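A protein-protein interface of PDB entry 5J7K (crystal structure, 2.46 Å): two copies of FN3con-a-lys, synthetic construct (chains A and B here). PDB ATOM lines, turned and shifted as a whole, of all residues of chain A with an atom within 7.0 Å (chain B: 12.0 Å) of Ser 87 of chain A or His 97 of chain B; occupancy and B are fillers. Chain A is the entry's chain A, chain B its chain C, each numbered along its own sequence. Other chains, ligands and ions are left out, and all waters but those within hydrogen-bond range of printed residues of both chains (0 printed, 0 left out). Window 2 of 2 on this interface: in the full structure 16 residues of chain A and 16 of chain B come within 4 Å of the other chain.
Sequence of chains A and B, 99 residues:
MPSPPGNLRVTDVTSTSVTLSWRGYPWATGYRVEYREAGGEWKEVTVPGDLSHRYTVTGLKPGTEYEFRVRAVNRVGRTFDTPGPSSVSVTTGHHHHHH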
ATOM      1  N   GLY A   6     -28.364  16.775  -2.327  1.00  0.00           N
ATOM      2  CA  GLY A   6     -28.120  16.441  -3.717  1.00  0.00           C
ATOM      3  C   GLY A   6     -27.345  15.151  -3.882  1.00  0.00           C
ATOM      4  O   GLY A   6     -26.135  15.162  -4.099  1.00  0.00           O
ATOM      5  N   LEU A   8     -26.083  11.595  -5.531  1.00  0.00           N
ATOM      6  CA  LEU A   8     -25.668  11.180  -6.859  1.00  0.00           C
ATOM      7  C   LEU A   8     -25.689   9.663  -6.841  1.00  0.00           C
ATOM      8  O   LEU A   8     -25.083   9.040  -5.963  1.00  0.00           O
ATOM      9  CB  LEU A   8     -24.278  11.727  -7.208  1.00  0.00           C
ATOM     10  CG  LEU A   8     -23.706  11.380  -8.584  1.00  0.00           C
ATOM     11  CD1 LEU A   8     -24.699  11.716  -9.671  1.00  0.00           C
ATOM     12  CD2 LEU A   8     -22.394  12.114  -8.816  1.00  0.00           C
ATOM     13  N   ARG A   9     -26.363   9.075  -7.820  1.00  0.00           N
ATOM     14  CA  ARG A   9     -26.665   7.657  -7.787  1.00  0.00           C
ATOM     15  C   ARG A   9     -26.132   6.983  -9.037  1.00  0.00           C
ATOM     16  O   ARG A   9     -26.196   7.541 -10.138  1.00  0.00           O
ATOM     17  CB  ARG A   9     -28.175   7.437  -7.692  1.00  0.00           C
ATOM     18  CG  ARG A   9     -28.866   8.260  -6.614  1.00  0.00           C
ATOM     19  CD  ARG A   9     -28.591   7.696  -5.233  1.00  0.00           C
ATOM     20  N   VAL A  10     -25.640   5.768  -8.862  1.00  0.00           N
ATOM     21  CA  VAL A  10     -25.107   4.979  -9.958  1.00  0.00           C
ATOM     22  C   VAL A  10     -26.135   3.893 -10.234  1.00  0.00           C
ATOM     23  O   VAL A  10     -26.278   2.950  -9.447  1.00  0.00           O
ATOM     24  CB  VAL A  10     -23.739   4.389  -9.595  1.00  0.00           C
ATOM     25  CG1 VAL A  10     -23.139   3.682 -10.773  1.00  0.00           C
ATOM     26  CG2 VAL A  10     -22.818   5.465  -9.048  1.00  0.00           C
ATOM     27  N   TRP A  42      -9.000  14.799 -15.967  1.00  0.00           N
ATOM     28  CA  TRP A  42     -10.411  15.158 -15.937  1.00  0.00           C
ATOM     29  C   TRP A  42     -10.927  15.393 -17.350  1.00  0.00           C
ATOM     30  O   TRP A  42     -10.263  16.037 -18.167  1.00  0.00           O
ATOM     31  CB  TRP A  42     -10.636  16.423 -15.109  1.00  0.00           C
ATOM     32  CG  TRP A  42     -10.449  16.279 -13.638  1.00  0.00           C
ATOM     33  CD1 TRP A  42      -9.408  16.750 -12.899  1.00  0.00           C
ATOM     34  CD2 TRP A  42     -11.340  15.641 -12.714  1.00  0.00           C
ATOM     35  NE1 TRP A  42      -9.587  16.442 -11.572  1.00  0.00           N
ATOM     36  CE2 TRP A  42     -10.766  15.758 -11.434  1.00  0.00           C
ATOM     37  CE3 TRP A  42     -12.561  14.974 -12.846  1.00  0.00           C
ATOM     38  CZ2 TRP A  42     -11.370  15.235 -10.294  1.00  0.00           C
ATOM     39  CZ3 TRP A  42     -13.159  14.455 -11.712  1.00  0.00           C
ATOM     40  CH2 TRP A  42     -12.565  14.589 -10.454  1.00  0.00           C
ATOM     41  N   GLU A  67     -13.477   8.423 -11.385  1.00  0.00           N
ATOM     42  CA  GLU A  67     -14.052   9.323 -10.401  1.00  0.00           C
ATOM     43  C   GLU A  67     -15.036  10.246 -11.101  1.00  0.00           C
ATOM     44  O   GLU A  67     -14.757  10.739 -12.196  1.00  0.00           O
ATOM     45  CB  GLU A  67     -12.956  10.124  -9.704  1.00  0.00           C
ATOM     46  CG  GLU A  67     -13.399  10.815  -8.440  1.00  0.00           C
ATOM     47  CD  GLU A  67     -12.222  11.361  -7.648  1.00  0.00           C
ATOM     48  OE1 GLU A  67     -11.136  10.752  -7.685  1.00  0.00           O
ATOM     49  OE2 GLU A  67     -12.373  12.405  -6.993  1.00  0.00           O
ATOM     50  N   PHE A  68     -16.189  10.465 -10.476  1.00  0.00           N
ATOM     51  CA  PHE A  68     -17.256  11.267 -11.061  1.00  0.00           C
ATOM     52  C   PHE A  68     -17.742  12.311 -10.070  1.00  0.00           C
ATOM     53  O   PHE A  68     -17.838  12.047  -8.868  1.00  0.00           O
ATOM     54  CB  PHE A  68     -18.463  10.423 -11.490  1.00  0.00           C
ATOM     55  CG  PHE A  68     -18.201   9.482 -12.627  1.00  0.00           C
ATOM     56  CD1 PHE A  68     -18.333   9.907 -13.937  1.00  0.00           C
ATOM     57  CD2 PHE A  68     -17.867   8.162 -12.389  1.00  0.00           C
ATOM     58  CE1 PHE A  68     -18.122   9.040 -14.983  1.00  0.00           C
ATOM     59  CE2 PHE A  68     -17.650   7.296 -13.430  1.00  0.00           C
ATOM     60  CZ  PHE A  68     -17.775   7.736 -14.728  1.00  0.00           C
ATOM     61  N   ARG A  69     -18.029  13.502 -10.585  1.00  0.00           N
ATOM     62  CA  ARG A  69     -18.703  14.541  -9.828  1.00  0.00           C
ATOM     63  C   ARG A  69     -19.561  15.317 -10.812  1.00  0.00           C
ATOM     64  O   ARG A  69     -19.185  15.486 -11.976  1.00  0.00           O
ATOM     65  CB  ARG A  69     -17.718  15.469  -9.117  1.00  0.00           C
ATOM     66  CG  ARG A  69     -16.867  16.262 -10.075  1.00  0.00           C
ATOM     67  CD  ARG A  69     -15.639  16.846  -9.414  1.00  0.00           C
ATOM     68  NE  ARG A  69     -14.857  17.599 -10.390  1.00  0.00           N
ATOM     69  CZ  ARG A  69     -13.646  18.096 -10.167  1.00  0.00           C
ATOM     70  NH1 ARG A  69     -13.062  17.921  -8.991  1.00  0.00           N
ATOM     71  NH2 ARG A  69     -13.020  18.766 -11.125  1.00  0.00           N
ATOM     72  N   VAL A  70     -20.716  15.778 -10.350  1.00  0.00           N
ATOM     73  CA  VAL A  70     -21.662  16.490 -11.198  1.00  0.00           C
ATOM     74  C   VAL A  70     -21.953  17.851 -10.588  1.00  0.00           C
ATOM     75  O   VAL A  70     -22.135  17.970  -9.372  1.00  0.00           O
ATOM     76  CB  VAL A  70     -22.965  15.684 -11.378  1.00  0.00           C
ATOM     77  CG1 VAL A  70     -24.014  16.522 -12.086  1.00  0.00           C
ATOM     78  CG2 VAL A  70     -22.691  14.402 -12.148  1.00  0.00           C
ATOM     79  N   PRO A  85     -20.132  19.753  -4.640  1.00  0.00           N
ATOM     80  CA  PRO A  85     -21.135  18.888  -5.269  1.00  0.00           C
ATOM     81  C   PRO A  85     -21.121  17.471  -4.705  1.00  0.00           C
ATOM     82  O   PRO A  85     -20.521  17.238  -3.657  1.00  0.00           O
ATOM     83  CB  PRO A  85     -20.719  18.887  -6.740  1.00  0.00           C
ATOM     84  CG  PRO A  85     -19.257  19.174  -6.716  1.00  0.00           C
ATOM     85  CD  PRO A  85     -19.061  20.130  -5.578  1.00  0.00           C
ATOM     86  N   SER A  86     -21.779  16.541  -5.388  1.00  0.00           N
ATOM     87  CA  SER A  86     -21.757  15.136  -5.006  1.00  0.00           C
ATOM     88  C   SER A  86     -20.778  14.376  -5.887  1.00  0.00           C
ATOM     89  O   SER A  86     -20.742  14.572  -7.107  1.00  0.00           O
ATOM     90  CB  SER A  86     -23.148  14.510  -5.107  1.00  0.00           C
ATOM     91  OG  SER A  86     -23.866  14.681  -3.895  1.00  0.00           O
ATOM     92  N   SER A  87     -19.986  13.505  -5.261  1.00  0.00           N
ATOM     93  CA  SER A  87     -18.907  12.787  -5.929  1.00  0.00           C
ATOM     94  C   SER A  87     -19.064  11.289  -5.707  1.00  0.00           C
ATOM     95  O   SER A  87     -19.441  10.850  -4.616  1.00  0.00           O
ATOM     96  CB  SER A  87     -17.540  13.255  -5.415  1.00  0.00           C
ATOM     97  OG  SER A  87     -16.508  12.861  -6.298  1.00  0.00           O
ATOM     98  N   VAL A  88     -18.784  10.505  -6.752  1.00  0.00           N
ATOM     99  CA  VAL A  88     -18.856   9.049  -6.691  1.00  0.00           C
ATOM    100  C   VAL A  88     -17.618   8.437  -7.346  1.00  0.00           C
ATOM    101  O   VAL A  88     -17.021   9.020  -8.256  1.00  0.00           O
ATOM    102  CB  VAL A  88     -20.159   8.532  -7.353  1.00  0.00           C
ATOM    103  CG1 VAL A  88     -20.176   8.856  -8.834  1.00  0.00           C
ATOM    104  CG2 VAL A  88     -20.345   7.045  -7.118  1.00  0.00           C
ATOM    105  N   SER A  89     -17.207   7.271  -6.842  1.00  0.00           N
ATOM    106  CA  SER A  89     -16.077   6.508  -7.368  1.00  0.00           C
ATOM    107  C   SER A  89     -16.582   5.203  -7.979  1.00  0.00           C
ATOM    108  O   SER A  89     -17.452   4.555  -7.401  1.00  0.00           O
ATOM    109  CB  SER A  89     -15.060   6.199  -6.260  1.00  0.00           C
ATOM    110  OG  SER A  89     -14.146   5.200  -6.678  1.00  0.00           O
ATOM    111  N   PRO B  62     -21.415  -7.430  -6.046  1.00  0.00           N
ATOM    112  CA  PRO B  62     -20.546  -6.469  -6.736  1.00  0.00           C
ATOM    113  C   PRO B  62     -19.094  -6.507  -6.276  1.00  0.00           C
ATOM    114  O   PRO B  62     -18.783  -6.792  -5.117  1.00  0.00           O
ATOM    115  CB  PRO B  62     -21.194  -5.115  -6.421  1.00  0.00           C
ATOM    116  CG  PRO B  62     -22.621  -5.431  -6.156  1.00  0.00           C
ATOM    117  CD  PRO B  62     -22.675  -6.821  -5.587  1.00  0.00           C
ATOM    118  N   GLY B  93     -18.697  -4.883 -10.962  1.00  0.00           N
ATOM    119  CA  GLY B  93     -18.410  -3.488 -10.710  1.00  0.00           C
ATOM    120  C   GLY B  93     -18.429  -3.121  -9.234  1.00  0.00           C
ATOM    121  O   GLY B  93     -19.026  -3.795  -8.394  1.00  0.00           O
ATOM    122  N   HIS B  94     -17.743  -2.013  -8.941  1.00  0.00           N
ATOM    123  CA  HIS B  94     -17.475  -1.487  -7.614  1.00  0.00           C
ATOM    124  C   HIS B  94     -17.747   0.015  -7.644  1.00  0.00           C
ATOM    125  O   HIS B  94     -17.495   0.663  -8.663  1.00  0.00           O
ATOM    126  CB  HIS B  94     -16.012  -1.856  -7.283  1.00  0.00           C
ATOM    127  CG  HIS B  94     -15.390  -1.083  -6.156  1.00  0.00           C
ATOM    128  ND1 HIS B  94     -14.112  -0.584  -6.241  1.00  0.00           N
ATOM    129  CD2 HIS B  94     -15.821  -0.793  -4.910  1.00  0.00           C
ATOM    130  CE1 HIS B  94     -13.797   0.017  -5.114  1.00  0.00           C
ATOM    131  NE2 HIS B  94     -14.813  -0.104  -4.288  1.00  0.00           N
ATOM    132  N   HIS B  95     -18.332   0.561  -6.572  1.00  0.00           N
ATOM    133  CA  HIS B  95     -18.585   2.002  -6.564  1.00  0.00           C
ATOM    134  C   HIS B  95     -18.873   2.531  -5.161  1.00  0.00           C
ATOM    135  O   HIS B  95     -19.464   1.840  -4.327  1.00  0.00           O
ATOM    136  CB  HIS B  95     -19.742   2.391  -7.498  1.00  0.00           C
ATOM    137  CG  HIS B  95     -21.101   2.058  -6.966  1.00  0.00           C
ATOM    138  ND1 HIS B  95     -21.653   2.690  -5.874  1.00  0.00           N
ATOM    139  CD2 HIS B  95     -22.033   1.181  -7.404  1.00  0.00           C
ATOM    140  CE1 HIS B  95     -22.852   2.190  -5.641  1.00  0.00           C
ATOM    141  NE2 HIS B  95     -23.114   1.283  -6.563  1.00  0.00           N
ATOM    142  N   HIS B  96     -18.465   3.784  -4.931  1.00  0.00           N
ATOM    143  CA  HIS B  96     -18.758   4.566  -3.716  1.00  0.00           C
ATOM    144  C   HIS B  96     -18.979   6.030  -4.104  1.00  0.00           C
ATOM    145  O   HIS B  96     -18.230   6.544  -4.926  1.00  0.00           O
ATOM    146  CB  HIS B  96     -17.606   4.515  -2.704  1.00  0.00           C
ATOM    147  CG  HIS B  96     -16.998   3.163  -2.511  1.00  0.00           C
ATOM    148  ND1 HIS B  96     -17.737   2.001  -2.479  1.00  0.00           N
ATOM    149  CD2 HIS B  96     -15.710   2.795  -2.317  1.00  0.00           C
ATOM    150  CE1 HIS B  96     -16.931   0.973  -2.285  1.00  0.00           C
ATOM    151  NE2 HIS B  96     -15.695   1.428  -2.178  1.00  0.00           N
ATOM    152  N   HIS B  97     -19.936   6.736  -3.504  1.00  0.00           N
ATOM    153  CA  HIS B  97     -20.758   6.256  -2.405  1.00  0.00           C
ATOM    154  C   HIS B  97     -22.199   6.103  -2.851  1.00  0.00           C
ATOM    155  O   HIS B  97     -22.840   7.079  -3.238  1.00  0.00           O
ATOM    156  CB  HIS B  97     -20.692   7.223  -1.227  1.00  0.00           C
ATOM    157  CG  HIS B  97     -19.346   7.843  -1.026  1.00  0.00           C
ATOM    158  ND1 HIS B  97     -18.471   7.413  -0.053  1.00  0.00           N
ATOM    159  CD2 HIS B  97     -18.725   8.864  -1.666  1.00  0.00           C
ATOM    160  CE1 HIS B  97     -17.368   8.139  -0.103  1.00  0.00           C
ATOM    161  NE2 HIS B  97     -17.496   9.026  -1.072  1.00  0.00           N
ATOM    162  N   HIS B  98     -22.695   4.875  -2.789  1.00  0.00           N
ATOM    163  CA  HIS B  98     -24.066   4.546  -3.153  1.00  0.00           C
ATOM    164  C   HIS B  98     -24.299   3.094  -2.776  1.00  0.00           C
ATOM    165  O   HIS B  98     -24.915   2.803  -1.749  1.00  0.00           O
ATOM    166  CB  HIS B  98     -24.304   4.786  -4.643  1.00  0.00           C
ATOM    167  CG  HIS B  98     -25.560   4.169  -5.189  1.00  0.00           C
ATOM    168  ND1 HIS B  98     -26.636   4.920  -5.608  1.00  0.00           N
ATOM    169  CD2 HIS B  98     -25.897   2.875  -5.409  1.00  0.00           C
ATOM    170  CE1 HIS B  98     -27.582   4.114  -6.061  1.00  0.00           C
ATOM    171  NE2 HIS B  98     -27.160   2.868  -5.948  1.00  0.00           N
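O of Ser 89 of chain A lies within hydrogen-bond range of N of His 96 of chain B (2.8 Å).
The backbone carbonyl oxygen of Phe 68 of chain A sits at hydrogen-bond distance from the side-chain hydroxyl of Ser 87 of chain A, 3.0 Å away. The backbone NH (N) of Phe 68 of chain A lies within hydrogen-bond range of the backbone carbonyl oxygen (O) of Val 88 of chain A (2.8 Å). A ring nitrogen (NE2) of His 94 of chain B lies within hydrogen-bond range of a ring nitrogen (NE2) of His 96 of chain B (2.8 Å).
Arg 9 of chain A touches His 98 of chain B (CD to ND1, 3.4 Å). Val 10 of chain A touches His 98 of chain B (N to ND1, 3.5 Å). O of Ser 87 of chain A touches CD2 of His 97 of chain B, at 3.6 Å. His 96 of chain B touches Val 88 of chain A. His 97 of chain B touches Val 88 of chain A (N to CG2, 3.7 Å). CA of His 95 of chain B touches O of Ser 89 of chain A (2.9 Å).
Of chain A, only Ser 87 and Val 88 come within 4 Å of His 97 of chain B. No residue of chain B comes within 4 Å of Leu 8 of chain A. Arg 9 of chain A touches just one residue of chain B: His 98 (3.4 Å). No residue of chain B comes within 4 Å of Glu 67 of chain A. No residue of chain B comes within 4 Å of Ser 86 of chain A. Of chain B, only His 96 (3.1 Å) and His 97 (3.7 Å) come within 4 Å of Val 88 of chain A. Of the printed residues of chain A, His 96 of chain B touches Val 88 (3.1 Å) and Ser 89 (2.3 Å). Printed residues of chain A within 4 Å of His 98 of chain B: Arg 9 (3.4 Å) and Val 10 (3.5 Å). Of the printed residues of chain A, His 95 of chain B touches Ser 89 (2.9 Å). Val 70 of chain A touches none of the printed residues of chain B. The nearest residue of chain B that does not touch Ser 87 of chain A is His 96 of chain B (4.5 Å). The nearest residue of chain A that does not touch His 97 of chain B is Leu 8 of chain A (4.04 Å). The nearest printed residue of chain A that does not touch His 98 of chain B is Leu 8 of chain A (4.4 Å).
Printed residues of chain A that touch a printed residue of chain B: Arg 9, Val 10, Ser 87, Val 88 and Ser 89. Hydrophobic or aromatic side chains of chain A that line the printed part of chain B: Val 88. Printed residues of chain B that touch a printed residue of chain A: His 95, His 96, His 97 and His 98. Hydrophobic or aromatic side chains of chain B within 4 Å of the printed part of chain A: His 95, His 97 and His 98.
No position is printed for both chains. Of the 7 pairs that touch across the chains among the printed residues, none has its exchanged pair printed and touching as well.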
